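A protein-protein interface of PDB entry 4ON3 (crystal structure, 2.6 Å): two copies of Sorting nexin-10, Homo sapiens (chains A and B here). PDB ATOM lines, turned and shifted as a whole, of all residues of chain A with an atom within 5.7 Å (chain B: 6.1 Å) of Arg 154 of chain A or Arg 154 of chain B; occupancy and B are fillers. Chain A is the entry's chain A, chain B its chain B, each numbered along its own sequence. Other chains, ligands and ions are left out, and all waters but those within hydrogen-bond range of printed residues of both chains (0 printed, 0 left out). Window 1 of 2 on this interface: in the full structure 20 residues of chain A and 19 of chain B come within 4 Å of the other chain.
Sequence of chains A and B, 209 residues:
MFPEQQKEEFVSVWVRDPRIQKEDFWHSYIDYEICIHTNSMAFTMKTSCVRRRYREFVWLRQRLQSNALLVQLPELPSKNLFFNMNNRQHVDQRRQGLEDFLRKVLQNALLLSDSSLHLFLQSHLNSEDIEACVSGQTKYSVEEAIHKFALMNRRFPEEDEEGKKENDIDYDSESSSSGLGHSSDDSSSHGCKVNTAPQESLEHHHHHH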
ATOM      1  N   MET A  45       8.257  -3.687 -24.205  1.00  0.00           N
ATOM      2  CA  MET A  45       8.330  -4.921 -23.445  1.00  0.00           C
ATOM      3  C   MET A  45       9.534  -5.655 -23.861  1.00  0.00           C
ATOM      4  O   MET A  45       9.806  -5.725 -25.029  1.00  0.00           O
ATOM      5  CB  MET A  45       7.107  -5.844 -23.736  1.00  0.00           C
ATOM      6  CG  MET A  45       5.774  -5.276 -23.245  1.00  0.00           C
ATOM      7  SD  MET A  45       5.798  -5.196 -21.453  1.00  0.00           S
ATOM      8  CE  MET A  45       4.879  -3.703 -21.044  1.00  0.00           C
ATOM      9  N   LYS A  46      10.218  -6.287 -22.928  1.00  0.00           N
ATOM     10  CA  LYS A  46      11.482  -6.929 -23.256  1.00  0.00           C
ATOM     11  C   LYS A  46      11.197  -8.313 -23.694  1.00  0.00           C
ATOM     12  O   LYS A  46      12.043  -8.966 -24.225  1.00  0.00           O
ATOM     13  CB  LYS A  46      12.450  -6.930 -22.072  1.00  0.00           C
ATOM     14  CG  LYS A  46      12.498  -5.668 -21.185  1.00  0.00           C
ATOM     15  CD  LYS A  46      13.376  -4.522 -21.668  1.00  0.00           C
ATOM     16  CE  LYS A  46      12.735  -3.829 -22.865  1.00  0.00           C
ATOM     17  NZ  LYS A  46      13.111  -2.372 -22.965  1.00  0.00           N
ATOM     18  N   THR A  47       9.991  -8.783 -23.416  1.00  0.00           N
ATOM     19  CA  THR A  47       9.494 -10.022 -24.024  1.00  0.00           C
ATOM     20  C   THR A  47       8.047  -9.876 -24.475  1.00  0.00           C
ATOM     21  O   THR A  47       7.270  -9.115 -23.858  1.00  0.00           O
ATOM     22  CB  THR A  47       9.572 -11.282 -23.120  1.00  0.00           C
ATOM     23  OG1 THR A  47       8.576 -11.233 -22.081  1.00  0.00           O
ATOM     24  CG2 THR A  47      10.945 -11.455 -22.537  1.00  0.00           C
ATOM     25  N   SER A  48       7.725 -10.601 -25.557  1.00  0.00           N
ATOM     26  CA  SER A  48       6.395 -10.640 -26.095  1.00  0.00           C
ATOM     27  C   SER A  48       6.248 -11.915 -26.909  1.00  0.00           C
ATOM     28  O   SER A  48       7.233 -12.379 -27.461  1.00  0.00           O
ATOM     29  CB  SER A  48       6.099  -9.371 -26.885  1.00  0.00           C
ATOM     30  OG  SER A  48       7.121  -9.014 -27.802  1.00  0.00           O
ATOM     31  N   PHE A 149      -2.028  -5.421 -23.407  1.00  0.00           N
ATOM     32  CA  PHE A 149      -1.836  -6.735 -23.984  1.00  0.00           C
ATOM     33  C   PHE A 149      -1.046  -7.617 -23.037  1.00  0.00           C
ATOM     34  O   PHE A 149      -1.391  -8.757 -22.823  1.00  0.00           O
ATOM     35  CB  PHE A 149      -1.056  -6.664 -25.290  1.00  0.00           C
ATOM     36  CG  PHE A 149      -0.770  -8.019 -25.894  1.00  0.00           C
ATOM     37  CD1 PHE A 149      -1.839  -8.937 -26.116  1.00  0.00           C
ATOM     38  CD2 PHE A 149       0.525  -8.373 -26.267  1.00  0.00           C
ATOM     39  CE1 PHE A 149      -1.604 -10.188 -26.668  1.00  0.00           C
ATOM     40  CE2 PHE A 149       0.783  -9.603 -26.838  1.00  0.00           C
ATOM     41  CZ  PHE A 149      -0.269 -10.520 -27.019  1.00  0.00           C
ATOM     42  N   ALA A 150       0.040  -7.068 -22.496  1.00  0.00           N
ATOM     43  CA  ALA A 150       0.954  -7.791 -21.628  1.00  0.00           C
ATOM     44  C   ALA A 150       0.251  -8.375 -20.420  1.00  0.00           C
ATOM     45  O   ALA A 150       0.369  -9.574 -20.149  1.00  0.00           O
ATOM     46  CB  ALA A 150       2.048  -6.860 -21.166  1.00  0.00           C
ATOM     47  N   LEU A 151      -0.447  -7.510 -19.687  1.00  0.00           N
ATOM     48  CA  LEU A 151      -1.350  -7.927 -18.615  1.00  0.00           C
ATOM     49  C   LEU A 151      -2.361  -9.026 -19.059  1.00  0.00           C
ATOM     50  O   LEU A 151      -2.413 -10.068 -18.411  1.00  0.00           O
ATOM     51  CB  LEU A 151      -2.094  -6.704 -18.049  1.00  0.00           C
ATOM     52  CG  LEU A 151      -1.294  -5.498 -17.543  1.00  0.00           C
ATOM     53  CD1 LEU A 151      -2.136  -4.273 -17.232  1.00  0.00           C
ATOM     54  CD2 LEU A 151      -0.543  -5.887 -16.310  1.00  0.00           C
ATOM     55  N   MET A 152      -3.156  -8.820 -20.126  1.00  0.00           N
ATOM     56  CA  MET A 152      -4.061  -9.891 -20.585  1.00  0.00           C
ATOM     57  C   MET A 152      -3.182 -11.125 -20.677  1.00  0.00           C
ATOM     58  O   MET A 152      -3.452 -12.156 -20.096  1.00  0.00           O
ATOM     59  CB  MET A 152      -4.692  -9.679 -21.985  1.00  0.00           C
ATOM     60  CG  MET A 152      -5.906  -8.741 -22.148  1.00  0.00           C
ATOM     61  SD  MET A 152      -6.225  -8.143 -23.884  1.00  0.00           S
ATOM     62  CE  MET A 152      -5.828  -9.586 -24.928  1.00  0.00           C
ATOM     63  N   ASN A 153      -2.100 -10.992 -21.411  1.00  0.00           N
ATOM     64  CA  ASN A 153      -1.384 -12.132 -21.951  1.00  0.00           C
ATOM     65  C   ASN A 153      -0.586 -12.906 -20.890  1.00  0.00           C
ATOM     66  O   ASN A 153      -0.372 -14.083 -21.003  1.00  0.00           O
ATOM     67  CB  ASN A 153      -0.502 -11.634 -23.107  1.00  0.00           C
ATOM     68  CG  ASN A 153      -0.113 -12.732 -24.063  1.00  0.00           C
ATOM     69  OD1 ASN A 153      -0.852 -13.684 -24.257  1.00  0.00           O
ATOM     70  ND2 ASN A 153       1.059 -12.593 -24.685  1.00  0.00           N
ATOM     71  N   ARG A 154      -0.182 -12.214 -19.840  1.00  0.00           N
ATOM     72  CA  ARG A 154       0.484 -12.802 -18.664  1.00  0.00           C
ATOM     73  C   ARG A 154      -0.522 -13.086 -17.550  1.00  0.00           C
ATOM     74  O   ARG A 154      -0.141 -13.423 -16.459  1.00  0.00           O
ATOM     75  CB  ARG A 154       1.584 -11.828 -18.143  1.00  0.00           C
ATOM     76  CG  ARG A 154       2.799 -11.776 -19.070  1.00  0.00           C
ATOM     77  CD  ARG A 154       3.582 -10.481 -18.993  1.00  0.00           C
ATOM     78  NE  ARG A 154       4.313 -10.236 -20.248  1.00  0.00           N
ATOM     79  CZ  ARG A 154       5.173  -9.223 -20.447  1.00  0.00           C
ATOM     80  NH1 ARG A 154       5.442  -8.350 -19.480  1.00  0.00           N
ATOM     81  NH2 ARG A 154       5.763  -9.063 -21.629  1.00  0.00           N
ATOM     82  N   ARG A 155      -1.812 -12.914 -17.814  1.00  0.00           N
ATOM     83  CA  ARG A 155      -2.853 -13.176 -16.822  1.00  0.00           C
ATOM     84  C   ARG A 155      -2.521 -12.461 -15.530  1.00  0.00           C
ATOM     85  O   ARG A 155      -2.576 -13.010 -14.466  1.00  0.00           O
ATOM     86  CB  ARG A 155      -3.016 -14.688 -16.608  1.00  0.00           C
ATOM     87  CG  ARG A 155      -3.237 -15.472 -17.900  1.00  0.00           C
ATOM     88  CD  ARG A 155      -3.019 -16.960 -17.685  1.00  0.00           C
ATOM     89  NE  ARG A 155      -4.289 -17.700 -17.691  1.00  0.00           N
ATOM     90  CZ  ARG A 155      -5.180 -17.784 -16.680  1.00  0.00           C
ATOM     91  NH1 ARG A 155      -4.991 -17.159 -15.516  1.00  0.00           N
ATOM     92  NH2 ARG A 155      -6.293 -18.511 -16.837  1.00  0.00           N
ATOM     93  N   PHE A 156      -2.178 -11.211 -15.637  1.00  0.00           N
ATOM     94  CA  PHE A 156      -1.750 -10.482 -14.469  1.00  0.00           C
ATOM     95  C   PHE A 156      -2.894 -10.239 -13.470  1.00  0.00           C
ATOM     96  O   PHE A 156      -3.961  -9.805 -13.870  1.00  0.00           O
ATOM     97  CB  PHE A 156      -1.193  -9.137 -14.924  1.00  0.00           C
ATOM     98  CG  PHE A 156      -0.201  -8.531 -13.979  1.00  0.00           C
ATOM     99  CD1 PHE A 156       1.128  -9.052 -13.909  1.00  0.00           C
ATOM    100  CD2 PHE A 156      -0.570  -7.437 -13.180  1.00  0.00           C
ATOM    101  CE1 PHE A 156       2.061  -8.489 -13.063  1.00  0.00           C
ATOM    102  CE2 PHE A 156       0.358  -6.867 -12.340  1.00  0.00           C
ATOM    103  CZ  PHE A 156       1.675  -7.394 -12.284  1.00  0.00           C
ATOM    104  N   PRO A 157      -2.673 -10.495 -12.158  1.00  0.00           N
ATOM    105  CA  PRO A 157      -3.712 -10.109 -11.179  1.00  0.00           C
ATOM    106  C   PRO A 157      -3.540  -8.687 -10.625  1.00  0.00           C
ATOM    107  O   PRO A 157      -4.145  -7.759 -11.160  1.00  0.00           O
ATOM    108  CB  PRO A 157      -3.559 -11.169 -10.074  1.00  0.00           C
ATOM    109  CG  PRO A 157      -2.364 -12.028 -10.443  1.00  0.00           C
ATOM    110  CD  PRO A 157      -1.625 -11.328 -11.530  1.00  0.00           C
ATOM    111  N   MET B  45      11.955  -5.102 -16.181  1.00  0.00           N
ATOM    112  CA  MET B  45      10.767  -5.739 -16.691  1.00  0.00           C
ATOM    113  C   MET B  45       9.581  -4.910 -16.312  1.00  0.00           C
ATOM    114  O   MET B  45       9.518  -4.397 -15.197  1.00  0.00           O
ATOM    115  CB  MET B  45      10.666  -7.117 -16.105  1.00  0.00           C
ATOM    116  CG  MET B  45      11.728  -8.023 -16.687  1.00  0.00           C
ATOM    117  SD  MET B  45      11.475  -8.273 -18.429  1.00  0.00           S
ATOM    118  CE  MET B  45      12.897  -9.292 -18.811  1.00  0.00           C
ATOM    119  N   LYS B  46       8.650  -4.734 -17.244  1.00  0.00           N
ATOM    120  CA  LYS B  46       7.533  -3.819 -16.996  1.00  0.00           C
ATOM    121  C   LYS B  46       6.428  -4.536 -16.201  1.00  0.00           C
ATOM    122  O   LYS B  46       5.553  -3.888 -15.646  1.00  0.00           O
ATOM    123  CB  LYS B  46       7.014  -3.235 -18.309  1.00  0.00           C
ATOM    124  CG  LYS B  46       8.101  -2.572 -19.135  1.00  0.00           C
ATOM    125  CD  LYS B  46       8.101  -1.050 -19.061  1.00  0.00           C
ATOM    126  CE  LYS B  46       9.411  -0.494 -19.611  1.00  0.00           C
ATOM    127  NZ  LYS B  46      10.445  -0.677 -18.529  1.00  0.00           N
ATOM    128  N   THR B  47       6.479  -5.863 -16.187  1.00  0.00           N
ATOM    129  CA  THR B  47       5.689  -6.625 -15.274  1.00  0.00           C
ATOM    130  C   THR B  47       6.533  -7.758 -14.759  1.00  0.00           C
ATOM    131  O   THR B  47       7.408  -8.224 -15.455  1.00  0.00           O
ATOM    132  CB  THR B  47       4.378  -7.233 -15.891  1.00  0.00           C
ATOM    133  OG1 THR B  47       4.668  -8.393 -16.674  1.00  0.00           O
ATOM    134  CG2 THR B  47       3.655  -6.264 -16.716  1.00  0.00           C
ATOM    135  N   SER B  48       6.218  -8.198 -13.543  1.00  0.00           N
ATOM    136  CA  SER B  48       6.868  -9.331 -12.912  1.00  0.00           C
ATOM    137  C   SER B  48       6.019  -9.962 -11.795  1.00  0.00           C
ATOM    138  O   SER B  48       5.386  -9.251 -11.022  1.00  0.00           O
ATOM    139  CB  SER B  48       8.207  -8.882 -12.355  1.00  0.00           C
ATOM    140  OG  SER B  48       8.020  -7.886 -11.369  1.00  0.00           O
ATOM    141  N   PHE B 149      14.711 -15.025 -15.850  1.00  0.00           N
ATOM    142  CA  PHE B 149      13.602 -15.349 -15.019  1.00  0.00           C
ATOM    143  C   PHE B 149      12.352 -15.110 -15.819  1.00  0.00           C
ATOM    144  O   PHE B 149      11.473 -15.952 -15.870  1.00  0.00           O
ATOM    145  CB  PHE B 149      13.557 -14.477 -13.801  1.00  0.00           C
ATOM    146  CG  PHE B 149      12.362 -14.719 -12.994  1.00  0.00           C
ATOM    147  CD1 PHE B 149      12.156 -15.993 -12.439  1.00  0.00           C
ATOM    148  CD2 PHE B 149      11.425 -13.736 -12.836  1.00  0.00           C
ATOM    149  CE1 PHE B 149      11.024 -16.273 -11.740  1.00  0.00           C
ATOM    150  CE2 PHE B 149      10.301 -13.976 -12.118  1.00  0.00           C
ATOM    151  CZ  PHE B 149      10.095 -15.247 -11.576  1.00  0.00           C
ATOM    152  N   ALA B 150      12.283 -13.942 -16.459  1.00  0.00           N
ATOM    153  CA  ALA B 150      11.195 -13.614 -17.385  1.00  0.00           C
ATOM    154  C   ALA B 150      10.999 -14.739 -18.384  1.00  0.00           C
ATOM    155  O   ALA B 150       9.929 -15.196 -18.559  1.00  0.00           O
ATOM    156  CB  ALA B 150      11.500 -12.327 -18.104  1.00  0.00           C
ATOM    157  N   LEU B 151      12.040 -15.216 -19.019  1.00  0.00           N
ATOM    158  CA  LEU B 151      11.883 -16.322 -19.946  1.00  0.00           C
ATOM    159  C   LEU B 151      11.466 -17.668 -19.309  1.00  0.00           C
ATOM    160  O   LEU B 151      10.674 -18.325 -19.930  1.00  0.00           O
ATOM    161  CB  LEU B 151      13.160 -16.526 -20.734  1.00  0.00           C
ATOM    162  CG  LEU B 151      13.773 -15.282 -21.364  1.00  0.00           C
ATOM    163  CD1 LEU B 151      15.159 -15.600 -21.875  1.00  0.00           C
ATOM    164  CD2 LEU B 151      12.891 -14.750 -22.479  1.00  0.00           C
ATOM    165  N   MET B 152      11.995 -18.091 -18.140  1.00  0.00           N
ATOM    166  CA  MET B 152      11.589 -19.349 -17.460  1.00  0.00           C
ATOM    167  C   MET B 152      10.094 -19.148 -17.215  1.00  0.00           C
ATOM    168  O   MET B 152       9.230 -19.994 -17.483  1.00  0.00           O
ATOM    169  CB  MET B 152      12.250 -19.571 -16.052  1.00  0.00           C
ATOM    170  CG  MET B 152      13.698 -20.148 -15.933  1.00  0.00           C
ATOM    171  SD  MET B 152      14.757 -19.779 -14.415  1.00  0.00           S
ATOM    172  CE  MET B 152      15.505 -21.386 -14.070  1.00  0.00           C
ATOM    173  N   ASN B 153       9.796 -17.970 -16.707  1.00  0.00           N
ATOM    174  CA  ASN B 153       8.549 -17.724 -16.083  1.00  0.00           C
ATOM    175  C   ASN B 153       7.423 -17.396 -17.057  1.00  0.00           C
ATOM    176  O   ASN B 153       6.313 -17.312 -16.635  1.00  0.00           O
ATOM    177  CB  ASN B 153       8.772 -16.572 -15.129  1.00  0.00           C
ATOM    178  CG  ASN B 153       7.760 -16.519 -14.044  1.00  0.00           C
ATOM    179  OD1 ASN B 153       7.434 -17.528 -13.420  1.00  0.00           O
ATOM    180  ND2 ASN B 153       7.265 -15.325 -13.779  1.00  0.00           N
ATOM    181  N   ARG B 154       7.686 -17.195 -18.345  1.00  0.00           N
ATOM    182  CA  ARG B 154       6.661 -16.759 -19.318  1.00  0.00           C
ATOM    183  C   ARG B 154       6.586 -17.856 -20.356  1.00  0.00           C
ATOM    184  O   ARG B 154       6.451 -17.622 -21.580  1.00  0.00           O
ATOM    185  CB  ARG B 154       7.061 -15.415 -19.968  1.00  0.00           C
ATOM    186  CG  ARG B 154       6.759 -14.208 -19.092  1.00  0.00           C
ATOM    187  CD  ARG B 154       7.384 -12.898 -19.558  1.00  0.00           C
ATOM    188  NE  ARG B 154       7.291 -11.885 -18.507  1.00  0.00           N
ATOM    189  CZ  ARG B 154       7.791 -10.645 -18.577  1.00  0.00           C
ATOM    190  NH1 ARG B 154       8.433 -10.217 -19.670  1.00  0.00           N
ATOM    191  NH2 ARG B 154       7.666  -9.814 -17.533  1.00  0.00           N
ATOM    192  N   ARG B 155       6.696 -19.070 -19.832  1.00  0.00           N
ATOM    193  CA  ARG B 155       7.231 -20.235 -20.550  1.00  0.00           C
ATOM    194  C   ARG B 155       7.676 -19.932 -21.972  1.00  0.00           C
ATOM    195  O   ARG B 155       7.229 -20.553 -22.914  1.00  0.00           O
ATOM    196  CB  ARG B 155       6.232 -21.378 -20.497  1.00  0.00           C
ATOM    197  CG  ARG B 155       6.218 -22.046 -19.139  1.00  0.00           C
ATOM    198  CD  ARG B 155       4.814 -22.427 -18.689  1.00  0.00           C
ATOM    199  NE  ARG B 155       4.857 -23.666 -17.902  1.00  0.00           N
ATOM    200  CZ  ARG B 155       3.893 -24.111 -17.101  1.00  0.00           C
ATOM    201  NH1 ARG B 155       2.765 -23.429 -16.949  1.00  0.00           N
ATOM    202  NH2 ARG B 155       4.070 -25.251 -16.446  1.00  0.00           N
ATOM    203  N   PHE B 156       8.588 -18.980 -22.098  1.00  0.00           N
ATOM    204  CA  PHE B 156       9.095 -18.581 -23.383  1.00  0.00           C
ATOM    205  C   PHE B 156       9.767 -19.758 -24.084  1.00  0.00           C
ATOM    206  O   PHE B 156      10.612 -20.426 -23.504  1.00  0.00           O
ATOM    207  CB  PHE B 156      10.125 -17.477 -23.210  1.00  0.00           C
ATOM    208  CG  PHE B 156      10.196 -16.504 -24.355  1.00  0.00           C
ATOM    209  CD1 PHE B 156       9.313 -15.404 -24.413  1.00  0.00           C
ATOM    210  CD2 PHE B 156      11.172 -16.641 -25.330  1.00  0.00           C
ATOM    211  CE1 PHE B 156       9.408 -14.471 -25.434  1.00  0.00           C
ATOM    212  CE2 PHE B 156      11.271 -15.715 -26.354  1.00  0.00           C
ATOM    213  CZ  PHE B 156      10.395 -14.628 -26.401  1.00  0.00           C
ATOM    214  N   PRO B 157       9.371 -20.022 -25.339  1.00  0.00           N
ATOM    215  CA  PRO B 157      10.065 -20.983 -26.215  1.00  0.00           C
ATOM    216  C   PRO B 157      11.606 -20.778 -26.321  1.00  0.00           C
ATOM    217  O   PRO B 157      12.078 -19.831 -26.984  1.00  0.00           O
ATOM    218  CB  PRO B 157       9.370 -20.767 -27.566  1.00  0.00           C
ATOM    219  CG  PRO B 157       7.974 -20.284 -27.222  1.00  0.00           C
ATOM    220  CD  PRO B 157       8.103 -19.529 -25.936  1.00  0.00           C
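Met 45 of chain A touches Lys 46 of chain B, and with the chains exchanged Lys 46 of chain A touches Met 45 of chain B. Thr 47 of chain A touches Leu 151 of chain B, but with the chains exchanged Leu 151 of chain A does not touch Thr 47 of chain B (4.2 Å). Thr 47 of chain A touches Arg 154 of chain B, and with the chains exchanged Arg 154 of chain A touches Thr 47 of chain B. Arg 154 of chain B touches its own counterpart, Arg 154 of chain A. 13 positions are printed for both chains. Of the 10 pairs that touch across the chains among the printed residues, 9 have their exchanged pair printed and touching as well.
Of chain B, only Thr 47 and Arg 154 come within 4 Å of Arg 154 of chain A. Printed residues of chain B within 4 Å of Ser 48 of chain A: Phe 156 (3.6 Å). Printed residues of chain B within 4 Å of Thr 47 of chain A: Leu 151, Arg 154 and Phe 156. The nearest residue of chain B that does not touch Arg 154 of chain A is Lys 46 of chain B (5.1 Å). The nearest printed residue of chain A that does not touch Leu 151 of chain B is Lys 46 of chain A (6.1 Å).
Among the printed residues, pairs that only touch across the chains: Met 45 of chain A with Lys 46 of chain B (3.5 Å), Ser 48 of chain A with Phe 156 of chain B (3.6 Å), Thr 47 of chain A with Leu 151 of chain B (3.8 Å), Phe 156 of chain A with Thr 47 of chain B (3.9 Å), Lys 46 of chain A with Met 45 of chain B (3.9 Å), Thr 47 of chain A with Phe 156 of chain B (3.9 Å) and Phe 156 of chain A with Ser 48 of chain B (3.98 Å).
The backbone carbonyl oxygen (O) of Leu 151 of chain A is in hydrogen-bond range of the backbone NH (N) of Phe 156 of chain A (3.0 Å). The guanidinium group (NH2) of Arg 154 of chain A sits at hydrogen-bond distance from the backbone carbonyl oxygen (O) of Thr 47 of chain A, at 2.7 Å. The side-chain sulfur (SD) of Met 45 of chain A is in hydrogen-bond range of the guanidinium group (NH1) of Arg 154 of chain A (3.7 Å). The backbone carbonyl oxygen (O) of Leu 151 of chain B is in hydrogen-bond range of the backbone NH (N) of Phe 156 of chain B, 3.1 Å away. NH2 of Arg 154 of chain B is in hydrogen-bond range of O of Thr 47 of chain B (2.6 Å).
Of the 13 printed residues of chain B, 7 touch a printed residue of chain A. Of the 13 printed residues of chain A, 6 touch a printed residue of chain B. Printed residues of chain A that touch a printed residue of chain B: Met 45, Lys 46, Thr 47, Ser 48, Arg 154 and Phe 156. Hydrophobic or aromatic side chains of chain A within 4 Å of the printed part of chain B: Met 45 and Phe 156. Along chain A the printed residues that touch a printed residue of chain B span positions 45 to 156.
NH1 of Arg 154 of chain A is in hydrogen-bond range of OG1 of Thr 47 of chain B (2.9 Å). The guanidinium group (NH1) of Arg 154 of chain B sits at hydrogen-bond distance from the side-chain hydroxyl (OG1) of Thr 47 of chain A, at 2.6 Å. NH1 of Arg 154 of chain A sits close to NH2 of Arg 154 of chain B (3.3 Å).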
